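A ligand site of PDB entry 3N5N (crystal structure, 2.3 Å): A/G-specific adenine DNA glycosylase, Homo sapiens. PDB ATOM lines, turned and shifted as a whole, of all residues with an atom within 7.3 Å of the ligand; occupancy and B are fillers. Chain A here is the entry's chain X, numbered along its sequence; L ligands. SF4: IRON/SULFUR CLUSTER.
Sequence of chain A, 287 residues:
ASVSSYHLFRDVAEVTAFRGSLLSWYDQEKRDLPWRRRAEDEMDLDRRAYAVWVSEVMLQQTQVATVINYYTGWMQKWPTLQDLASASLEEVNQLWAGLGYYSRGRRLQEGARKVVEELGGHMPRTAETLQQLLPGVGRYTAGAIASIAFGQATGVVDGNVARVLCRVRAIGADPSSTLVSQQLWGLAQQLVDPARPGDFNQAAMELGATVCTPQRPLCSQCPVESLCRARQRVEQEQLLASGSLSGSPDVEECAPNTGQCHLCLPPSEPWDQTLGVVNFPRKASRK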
ATOM      1  N   PHE A  18      -0.219 -12.988   6.045  1.00  0.00           N
ATOM      2  CA  PHE A  18       0.298 -13.545   4.817  1.00  0.00           C
ATOM      3  C   PHE A  18       1.795 -13.862   5.013  1.00  0.00           C
ATOM      4  O   PHE A  18       2.250 -14.980   4.723  1.00  0.00           O
ATOM      5  CB  PHE A  18       0.104 -12.564   3.655  1.00  0.00           C
ATOM      6  CG  PHE A  18       0.345 -13.181   2.311  1.00  0.00           C
ATOM      7  CD1 PHE A  18       1.616 -13.245   1.779  1.00  0.00           C
ATOM      8  CD2 PHE A  18      -0.718 -13.702   1.584  1.00  0.00           C
ATOM      9  CE1 PHE A  18       1.826 -13.833   0.503  1.00  0.00           C
ATOM     10  CE2 PHE A  18      -0.503 -14.289   0.332  1.00  0.00           C
ATOM     11  CZ  PHE A  18       0.774 -14.340  -0.202  1.00  0.00           C
ATOM     12  N   ARG A 163       1.618 -15.835 -10.713  1.00  0.00           N
ATOM     13  CA  ARG A 163       0.498 -16.748 -10.687  1.00  0.00           C
ATOM     14  C   ARG A 163      -0.118 -16.661  -9.285  1.00  0.00           C
ATOM     15  O   ARG A 163      -1.320 -16.474  -9.149  1.00  0.00           O
ATOM     16  CB  ARG A 163       0.943 -18.178 -11.032  1.00  0.00           C
ATOM     17  CG  ARG A 163      -0.165 -19.195 -10.993  1.00  0.00           C
ATOM     18  CD  ARG A 163       0.283 -20.506 -11.610  1.00  0.00           C
ATOM     19  NE  ARG A 163       1.555 -20.924 -11.073  1.00  0.00           N
ATOM     20  CZ  ARG A 163       2.716 -20.759 -11.700  1.00  0.00           C
ATOM     21  NH1 ARG A 163       2.746 -20.194 -12.895  1.00  0.00           N
ATOM     22  NH2 ARG A 163       3.855 -21.165 -11.142  1.00  0.00           N
ATOM     23  N   VAL A 164       0.716 -16.762  -8.254  1.00  0.00           N
ATOM     24  CA  VAL A 164       0.207 -16.660  -6.868  1.00  0.00           C
ATOM     25  C   VAL A 164      -0.554 -15.356  -6.562  1.00  0.00           C
ATOM     26  O   VAL A 164      -1.680 -15.391  -6.076  1.00  0.00           O
ATOM     27  CB  VAL A 164       1.318 -16.821  -5.801  1.00  0.00           C
ATOM     28  CG1 VAL A 164       0.774 -16.553  -4.445  1.00  0.00           C
ATOM     29  CG2 VAL A 164       1.896 -18.189  -5.825  1.00  0.00           C
ATOM     30  N   LEU A 165       0.054 -14.213  -6.857  1.00  0.00           N
ATOM     31  CA  LEU A 165      -0.581 -12.928  -6.583  1.00  0.00           C
ATOM     32  C   LEU A 165      -1.875 -12.720  -7.394  1.00  0.00           C
ATOM     33  O   LEU A 165      -2.839 -12.111  -6.905  1.00  0.00           O
ATOM     34  CB  LEU A 165       0.407 -11.768  -6.821  1.00  0.00           C
ATOM     35  CG  LEU A 165       1.593 -11.641  -5.858  1.00  0.00           C
ATOM     36  CD1 LEU A 165       2.411 -10.490  -6.305  1.00  0.00           C
ATOM     37  CD2 LEU A 165       1.072 -11.386  -4.399  1.00  0.00           C
ATOM     38  N   ARG A 167      -3.944 -14.933  -8.185  1.00  0.00           N
ATOM     39  CA  ARG A 167      -4.980 -15.725  -7.583  1.00  0.00           C
ATOM     40  C   ARG A 167      -5.354 -15.130  -6.242  1.00  0.00           C
ATOM     41  O   ARG A 167      -6.527 -14.915  -5.967  1.00  0.00           O
ATOM     42  CB  ARG A 167      -4.561 -17.198  -7.494  1.00  0.00           C
ATOM     43  CG  ARG A 167      -4.541 -17.852  -8.889  1.00  0.00           C
ATOM     44  CD  ARG A 167      -3.772 -19.136  -8.950  1.00  0.00           C
ATOM     45  NE  ARG A 167      -3.967 -19.780 -10.256  1.00  0.00           N
ATOM     46  CZ  ARG A 167      -3.408 -20.935 -10.617  1.00  0.00           C
ATOM     47  NH1 ARG A 167      -2.630 -21.583  -9.754  1.00  0.00           N
ATOM     48  NH2 ARG A 167      -3.642 -21.451 -11.830  1.00  0.00           N
ATOM     49  N   VAL A 168      -4.344 -14.844  -5.417  1.00  0.00           N
ATOM     50  CA  VAL A 168      -4.556 -14.266  -4.098  1.00  0.00           C
ATOM     51  C   VAL A 168      -5.402 -12.971  -4.087  1.00  0.00           C
ATOM     52  O   VAL A 168      -6.155 -12.722  -3.166  1.00  0.00           O
ATOM     53  CB  VAL A 168      -3.206 -14.018  -3.351  1.00  0.00           C
ATOM     54  CG1 VAL A 168      -3.437 -13.126  -2.181  1.00  0.00           C
ATOM     55  CG2 VAL A 168      -2.638 -15.322  -2.882  1.00  0.00           C
ATOM     56  N   LEU A 207       6.057 -21.435  -3.440  1.00  0.00           N
ATOM     57  CA  LEU A 207       4.628 -21.688  -3.382  1.00  0.00           C
ATOM     58  C   LEU A 207       4.131 -21.841  -4.815  1.00  0.00           C
ATOM     59  O   LEU A 207       3.356 -22.748  -5.122  1.00  0.00           O
ATOM     60  CB  LEU A 207       3.934 -20.509  -2.673  1.00  0.00           C
ATOM     61  CG  LEU A 207       2.634 -20.668  -1.919  1.00  0.00           C
ATOM     62  CD1 LEU A 207       1.455 -19.869  -2.375  1.00  0.00           C
ATOM     63  CD2 LEU A 207       2.293 -22.079  -1.437  1.00  0.00           C
ATOM     64  N   VAL A 211       2.965 -25.615  -4.827  1.00  0.00           N
ATOM     65  CA  VAL A 211       1.560 -25.685  -4.462  1.00  0.00           C
ATOM     66  C   VAL A 211       0.624 -25.011  -5.463  1.00  0.00           C
ATOM     67  O   VAL A 211      -0.345 -25.631  -5.923  1.00  0.00           O
ATOM     68  CB  VAL A 211       1.316 -25.069  -3.071  1.00  0.00           C
ATOM     69  CG1 VAL A 211      -0.149 -25.181  -2.687  1.00  0.00           C
ATOM     70  CG2 VAL A 211       2.199 -25.739  -2.030  1.00  0.00           C
ATOM     71  N   CYS A 212       0.897 -23.761  -5.795  1.00  0.00           N
ATOM     72  CA  CYS A 212      -0.011 -22.982  -6.604  1.00  0.00           C
ATOM     73  C   CYS A 212       0.428 -23.097  -8.083  1.00  0.00           C
ATOM     74  O   CYS A 212       0.812 -22.118  -8.725  1.00  0.00           O
ATOM     75  CB  CYS A 212      -0.023 -21.541  -6.126  1.00  0.00           C
ATOM     76  SG  CYS A 212      -1.372 -20.544  -6.802  1.00  0.00           S
ATOM     77  N   THR A 213       0.368 -24.304  -8.607  1.00  0.00           N
ATOM     78  CA  THR A 213       0.851 -24.611  -9.927  1.00  0.00           C
ATOM     79  C   THR A 213      -0.058 -24.166 -11.069  1.00  0.00           C
ATOM     80  O   THR A 213      -1.241 -23.901 -10.855  1.00  0.00           O
ATOM     81  CB  THR A 213       1.090 -26.078 -10.032  1.00  0.00           C
ATOM     82  OG1 THR A 213      -0.136 -26.760  -9.685  1.00  0.00           O
ATOM     83  CG2 THR A 213       2.171 -26.492  -9.055  1.00  0.00           C
ATOM     84  N   PRO A 217      -3.856 -26.785  -8.773  1.00  0.00           N
ATOM     85  CA  PRO A 217      -3.156 -26.269  -7.580  1.00  0.00           C
ATOM     86  C   PRO A 217      -3.596 -26.973  -6.289  1.00  0.00           C
ATOM     87  O   PRO A 217      -4.728 -27.343  -6.160  1.00  0.00           O
ATOM     88  CB  PRO A 217      -3.571 -24.790  -7.541  1.00  0.00           C
ATOM     89  CG  PRO A 217      -4.872 -24.759  -8.311  1.00  0.00           C
ATOM     90  CD  PRO A 217      -4.726 -25.767  -9.388  1.00  0.00           C
ATOM     91  N   LEU A 218      -2.679 -27.121  -5.343  1.00  0.00           N
ATOM     92  CA  LEU A 218      -2.983 -27.809  -4.083  1.00  0.00           C
ATOM     93  C   LEU A 218      -3.507 -26.860  -3.020  1.00  0.00           C
ATOM     94  O   LEU A 218      -2.871 -26.675  -1.979  1.00  0.00           O
ATOM     95  CB  LEU A 218      -1.739 -28.529  -3.580  1.00  0.00           C
ATOM     96  CG  LEU A 218      -1.200 -29.589  -4.547  1.00  0.00           C
ATOM     97  CD1 LEU A 218      -1.241 -29.067  -5.960  1.00  0.00           C
ATOM     98  CD2 LEU A 218       0.223 -30.038  -4.172  1.00  0.00           C
ATOM     99  N   CYS A 219      -4.666 -26.268  -3.270  1.00  0.00           N
ATOM    100  CA  CYS A 219      -5.268 -25.308  -2.328  1.00  0.00           C
ATOM    101  C   CYS A 219      -5.506 -25.829  -0.924  1.00  0.00           C
ATOM    102  O   CYS A 219      -5.553 -25.051   0.012  1.00  0.00           O
ATOM    103  CB  CYS A 219      -6.579 -24.799  -2.884  1.00  0.00           C
ATOM    104  SG  CYS A 219      -6.415 -24.102  -4.494  1.00  0.00           S
ATOM    105  N   SER A 220      -5.702 -27.126  -0.771  1.00  0.00           N
ATOM    106  CA  SER A 220      -5.966 -27.684   0.560  1.00  0.00           C
ATOM    107  C   SER A 220      -4.697 -27.765   1.376  1.00  0.00           C
ATOM    108  O   SER A 220      -4.732 -27.892   2.593  1.00  0.00           O
ATOM    109  CB  SER A 220      -6.678 -29.061   0.484  1.00  0.00           C
ATOM    110  OG  SER A 220      -5.895 -29.999  -0.227  1.00  0.00           O
ATOM    111  N   GLN A 221      -3.557 -27.682   0.702  1.00  0.00           N
ATOM    112  CA  GLN A 221      -2.281 -27.704   1.398  1.00  0.00           C
ATOM    113  C   GLN A 221      -1.628 -26.366   1.393  1.00  0.00           C
ATOM    114  O   GLN A 221      -0.535 -26.209   1.906  1.00  0.00           O
ATOM    115  CB  GLN A 221      -1.376 -28.756   0.806  1.00  0.00           C
ATOM    116  CG  GLN A 221      -1.927 -30.172   1.034  1.00  0.00           C
ATOM    117  CD  GLN A 221      -1.120 -31.241   0.347  1.00  0.00           C
ATOM    118  OE1 GLN A 221      -0.473 -30.992  -0.667  1.00  0.00           O
ATOM    119  NE2 GLN A 221      -1.145 -32.444   0.907  1.00  0.00           N
ATOM    120  N   CYS A 222      -2.304 -25.369   0.823  1.00  0.00           N
ATOM    121  CA  CYS A 222      -1.765 -24.028   0.700  1.00  0.00           C
ATOM    122  C   CYS A 222      -1.796 -23.263   2.023  1.00  0.00           C
ATOM    123  O   CYS A 222      -2.818 -23.198   2.667  1.00  0.00           O
ATOM    124  CB  CYS A 222      -2.523 -23.268  -0.368  1.00  0.00           C
ATOM    125  SG  CYS A 222      -1.922 -21.608  -0.572  1.00  0.00           S
ATOM    126  N   PRO A 223      -0.674 -22.685   2.417  1.00  0.00           N
ATOM    127  CA  PRO A 223      -0.599 -21.991   3.714  1.00  0.00           C
ATOM    128  C   PRO A 223      -1.311 -20.659   3.673  1.00  0.00           C
ATOM    129  O   PRO A 223      -1.456 -19.998   4.702  1.00  0.00           O
ATOM    130  CB  PRO A 223       0.910 -21.779   3.912  1.00  0.00           C
ATOM    131  CG  PRO A 223       1.452 -21.703   2.517  1.00  0.00           C
ATOM    132  CD  PRO A 223       0.630 -22.763   1.761  1.00  0.00           C
ATOM    133  N   VAL A 224      -1.749 -20.286   2.500  1.00  0.00           N
ATOM    134  CA  VAL A 224      -2.326 -19.002   2.280  1.00  0.00           C
ATOM    135  C   VAL A 224      -3.790 -19.077   1.788  1.00  0.00           C
ATOM    136  O   VAL A 224      -4.387 -18.069   1.388  1.00  0.00           O
ATOM    137  CB  VAL A 224      -1.417 -18.267   1.282  1.00  0.00           C
ATOM    138  CG1 VAL A 224      -2.152 -17.610   0.204  1.00  0.00           C
ATOM    139  CG2 VAL A 224      -0.399 -17.372   2.008  1.00  0.00           C
ATOM    140  N   GLU A 225      -4.375 -20.266   1.858  1.00  0.00           N
ATOM    141  CA  GLU A 225      -5.756 -20.493   1.410  1.00  0.00           C
ATOM    142  C   GLU A 225      -6.772 -19.493   1.953  1.00  0.00           C
ATOM    143  O   GLU A 225      -7.610 -18.997   1.221  1.00  0.00           O
ATOM    144  CB  GLU A 225      -6.203 -21.892   1.757  1.00  0.00           C
ATOM    145  CG  GLU A 225      -7.589 -22.217   1.255  1.00  0.00           C
ATOM    146  CD  GLU A 225      -8.002 -23.635   1.561  1.00  0.00           C
ATOM    147  OE1 GLU A 225      -8.368 -24.370   0.618  1.00  0.00           O
ATOM    148  OE2 GLU A 225      -7.933 -24.034   2.750  1.00  0.00           O
ATOM    149  N   SER A 226      -6.697 -19.203   3.229  1.00  0.00           N
ATOM    150  CA  SER A 226      -7.643 -18.291   3.864  1.00  0.00           C
ATOM    151  C   SER A 226      -7.698 -16.910   3.278  1.00  0.00           C
ATOM    152  O   SER A 226      -8.746 -16.294   3.229  1.00  0.00           O
ATOM    153  CB  SER A 226      -7.359 -18.173   5.341  1.00  0.00           C
ATOM    154  OG  SER A 226      -7.745 -19.344   5.985  1.00  0.00           O
ATOM    155  N   LEU A 227      -6.557 -16.396   2.850  1.00  0.00           N
ATOM    156  CA  LEU A 227      -6.486 -15.049   2.359  1.00  0.00           C
ATOM    157  C   LEU A 227      -6.558 -15.015   0.830  1.00  0.00           C
ATOM    158  O   LEU A 227      -6.335 -13.973   0.209  1.00  0.00           O
ATOM    159  CB  LEU A 227      -5.180 -14.427   2.798  1.00  0.00           C
ATOM    160  CG  LEU A 227      -4.815 -14.713   4.232  1.00  0.00           C
ATOM    161  CD1 LEU A 227      -3.396 -14.306   4.507  1.00  0.00           C
ATOM    162  CD2 LEU A 227      -5.790 -14.011   5.181  1.00  0.00           C
ATOM    163  N   CYS A 228      -6.850 -16.157   0.226  1.00  0.00           N
ATOM    164  CA  CYS A 228      -6.821 -16.225  -1.218  1.00  0.00           C
ATOM    165  C   CYS A 228      -8.153 -15.892  -1.835  1.00  0.00           C
ATOM    166  O   CYS A 228      -9.098 -16.692  -1.793  1.00  0.00           O
ATOM    167  CB  CYS A 228      -6.356 -17.579  -1.690  1.00  0.00           C
ATOM    168  SG  CYS A 228      -6.238 -17.656  -3.459  1.00  0.00           S
ATOM    169  N   ARG A 229      -8.215 -14.725  -2.421  1.00  0.00           N
ATOM    170  CA  ARG A 229      -9.407 -14.266  -3.040  1.00  0.00           C
ATOM    171  C   ARG A 229      -9.981 -15.264  -4.071  1.00  0.00           C
ATOM    172  O   ARG A 229     -11.179 -15.499  -4.082  1.00  0.00           O
ATOM    173  CB  ARG A 229      -9.163 -12.886  -3.609  1.00  0.00           C
ATOM    174  CG  ARG A 229     -10.393 -12.122  -3.894  1.00  0.00           C
ATOM    175  CD  ARG A 229     -10.290 -10.778  -3.242  1.00  0.00           C
ATOM    176  NE  ARG A 229     -10.162 -10.962  -1.800  1.00  0.00           N
ATOM    177  CZ  ARG A 229     -10.040  -9.984  -0.915  1.00  0.00           C
ATOM    178  NH1 ARG A 229     -10.029  -8.716  -1.311  1.00  0.00           N
ATOM    179  NH2 ARG A 229      -9.929 -10.280   0.379  1.00  0.00           N
ATOM    180  N   ALA A 230      -9.157 -15.858  -4.922  1.00  0.00           N
ATOM    181  CA  ALA A 230      -9.704 -16.816  -5.910  1.00  0.00           C
ATOM    182  C   ALA A 230     -10.273 -18.034  -5.211  1.00  0.00           C
ATOM    183  O   ALA A 230     -11.346 -18.492  -5.532  1.00  0.00           O
ATOM    184  CB  ALA A 230      -8.643 -17.222  -6.929  1.00  0.00           C
ATOM    185  N   ARG A 231      -9.541 -18.563  -4.237  1.00  0.00           N
ATOM    186  CA  ARG A 231     -10.006 -19.699  -3.459  1.00  0.00           C
ATOM    187  C   ARG A 231     -11.379 -19.430  -2.806  1.00  0.00           C
ATOM    188  O   ARG A 231     -12.304 -20.228  -2.928  1.00  0.00           O
ATOM    189  CB  ARG A 231      -8.935 -20.112  -2.442  1.00  0.00           C
ATOM    190  CG  ARG A 231      -9.373 -21.111  -1.403  1.00  0.00           C
ATOM    191  CD  ARG A 231      -9.802 -22.384  -2.039  1.00  0.00           C
ATOM    192  NE  ARG A 231     -10.240 -23.359  -1.050  1.00  0.00           N
ATOM    193  CZ  ARG A 231     -10.886 -24.477  -1.363  1.00  0.00           C
ATOM    194  NH1 ARG A 231     -11.163 -24.749  -2.632  1.00  0.00           N
ATOM    195  NH2 ARG A 231     -11.260 -25.321  -0.413  1.00  0.00           N
ATOM    196  N   GLN A 232     -11.507 -18.301  -2.117  1.00  0.00           N
ATOM    197  CA  GLN A 232     -12.770 -17.953  -1.449  1.00  0.00           C
ATOM    198  C   GLN A 232     -13.913 -18.004  -2.461  1.00  0.00           C
ATOM    199  O   GLN A 232     -15.009 -18.509  -2.177  1.00  0.00           O
ATOM    200  CB  GLN A 232     -12.694 -16.543  -0.852  1.00  0.00           C
ATOM    201  CG  GLN A 232     -11.656 -16.363   0.276  1.00  0.00           C
ATOM    202  CD  GLN A 232     -11.235 -14.868   0.493  1.00  0.00           C
ATOM    203  OE1 GLN A 232     -11.763 -13.967  -0.153  1.00  0.00           O
ATOM    204  NE2 GLN A 232     -10.271 -14.647   1.389  1.00  0.00           N
HETATM  205 FE1  SF4 L   1      -3.144 -21.221  -2.504  1.00  0.00          FE
HETATM  206 FE2  SF4 L   1      -2.931 -20.593  -5.056  1.00  0.00          FE
HETATM  207 FE3  SF4 L   1      -4.948 -22.213  -4.253  1.00  0.00          FE
HETATM  208 FE4  SF4 L   1      -4.929 -19.517  -3.644  1.00  0.00          FE
HETATM  209  S1  SF4 L   1      -5.086 -20.471  -5.764  1.00  0.00           S
HETATM  210  S2  SF4 L   1      -5.417 -21.296  -2.210  1.00  0.00           S
HETATM  211  S3  SF4 L   1      -2.736 -19.110  -3.278  1.00  0.00           S
HETATM  212  S4  SF4 L   1      -2.726 -22.718  -4.222  1.00  0.00           S
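An iron atom (FE4) of the ligand is bound by the side-chain sulfur (SG) of Cys 228 (2.3 Å). The side-chain sulfur (SG) of Cys 219 binds an iron atom (FE3) of the ligand, at 2.4 Å. An iron atom (FE2) of the ligand is bound by the side-chain sulfur (SG) of Cys 212 (2.3 Å). SG of Cys 222 is bound to FE1 of the ligand.
The guanidinium group (NH1) of Arg 167 lies close to the side-chain sulfur (SG) of Cys 212, at 3.4 Å. The side-chain sulfur (SG) of Cys 228 lies close to the backbone NH (N) of Arg 231 (3.5 Å). The backbone NH of Ala 230 sits close to the side-chain sulfur of Cys 228 (3.7 Å). O of Thr 213 lies within hydrogen-bond range of NH1 of Arg 167, 2.9 Å away. O of Val 168 is in hydrogen-bond range of N of Arg 229, 3.0 Å away. The backbone carbonyl oxygen (O) of Arg 167 sits close to the side-chain sulfur (SG) of Cys 228 (3.7 Å). SG of Cys 222 lies close to N of Val 224, at 3.3 Å. N of Cys 212 is in hydrogen-bond range of O of Leu 207, 2.7 Å away.
CD of Arg 167 touches S1 of the ligand (3.7 Å). Val 168 touches the ligand. CG1 of Val 211 touches S4 of the ligand, 3.9 Å away. Val 224 touches the ligand (CG1 to S3, 3.8 Å). Glu 225 touches the ligand (CA to S2, 3.7 Å). Arg 231 touches the ligand (CB to S2, 3.7 Å). Within 4 Å of the ligand: Arg 167, Val 168, Val 211, Cys 212, Cys 219, Cys 222, Val 224, Glu 225, Cys 228 and Arg 231. Along chain A the residues within 4 Å of the ligand span positions 167 to 231.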
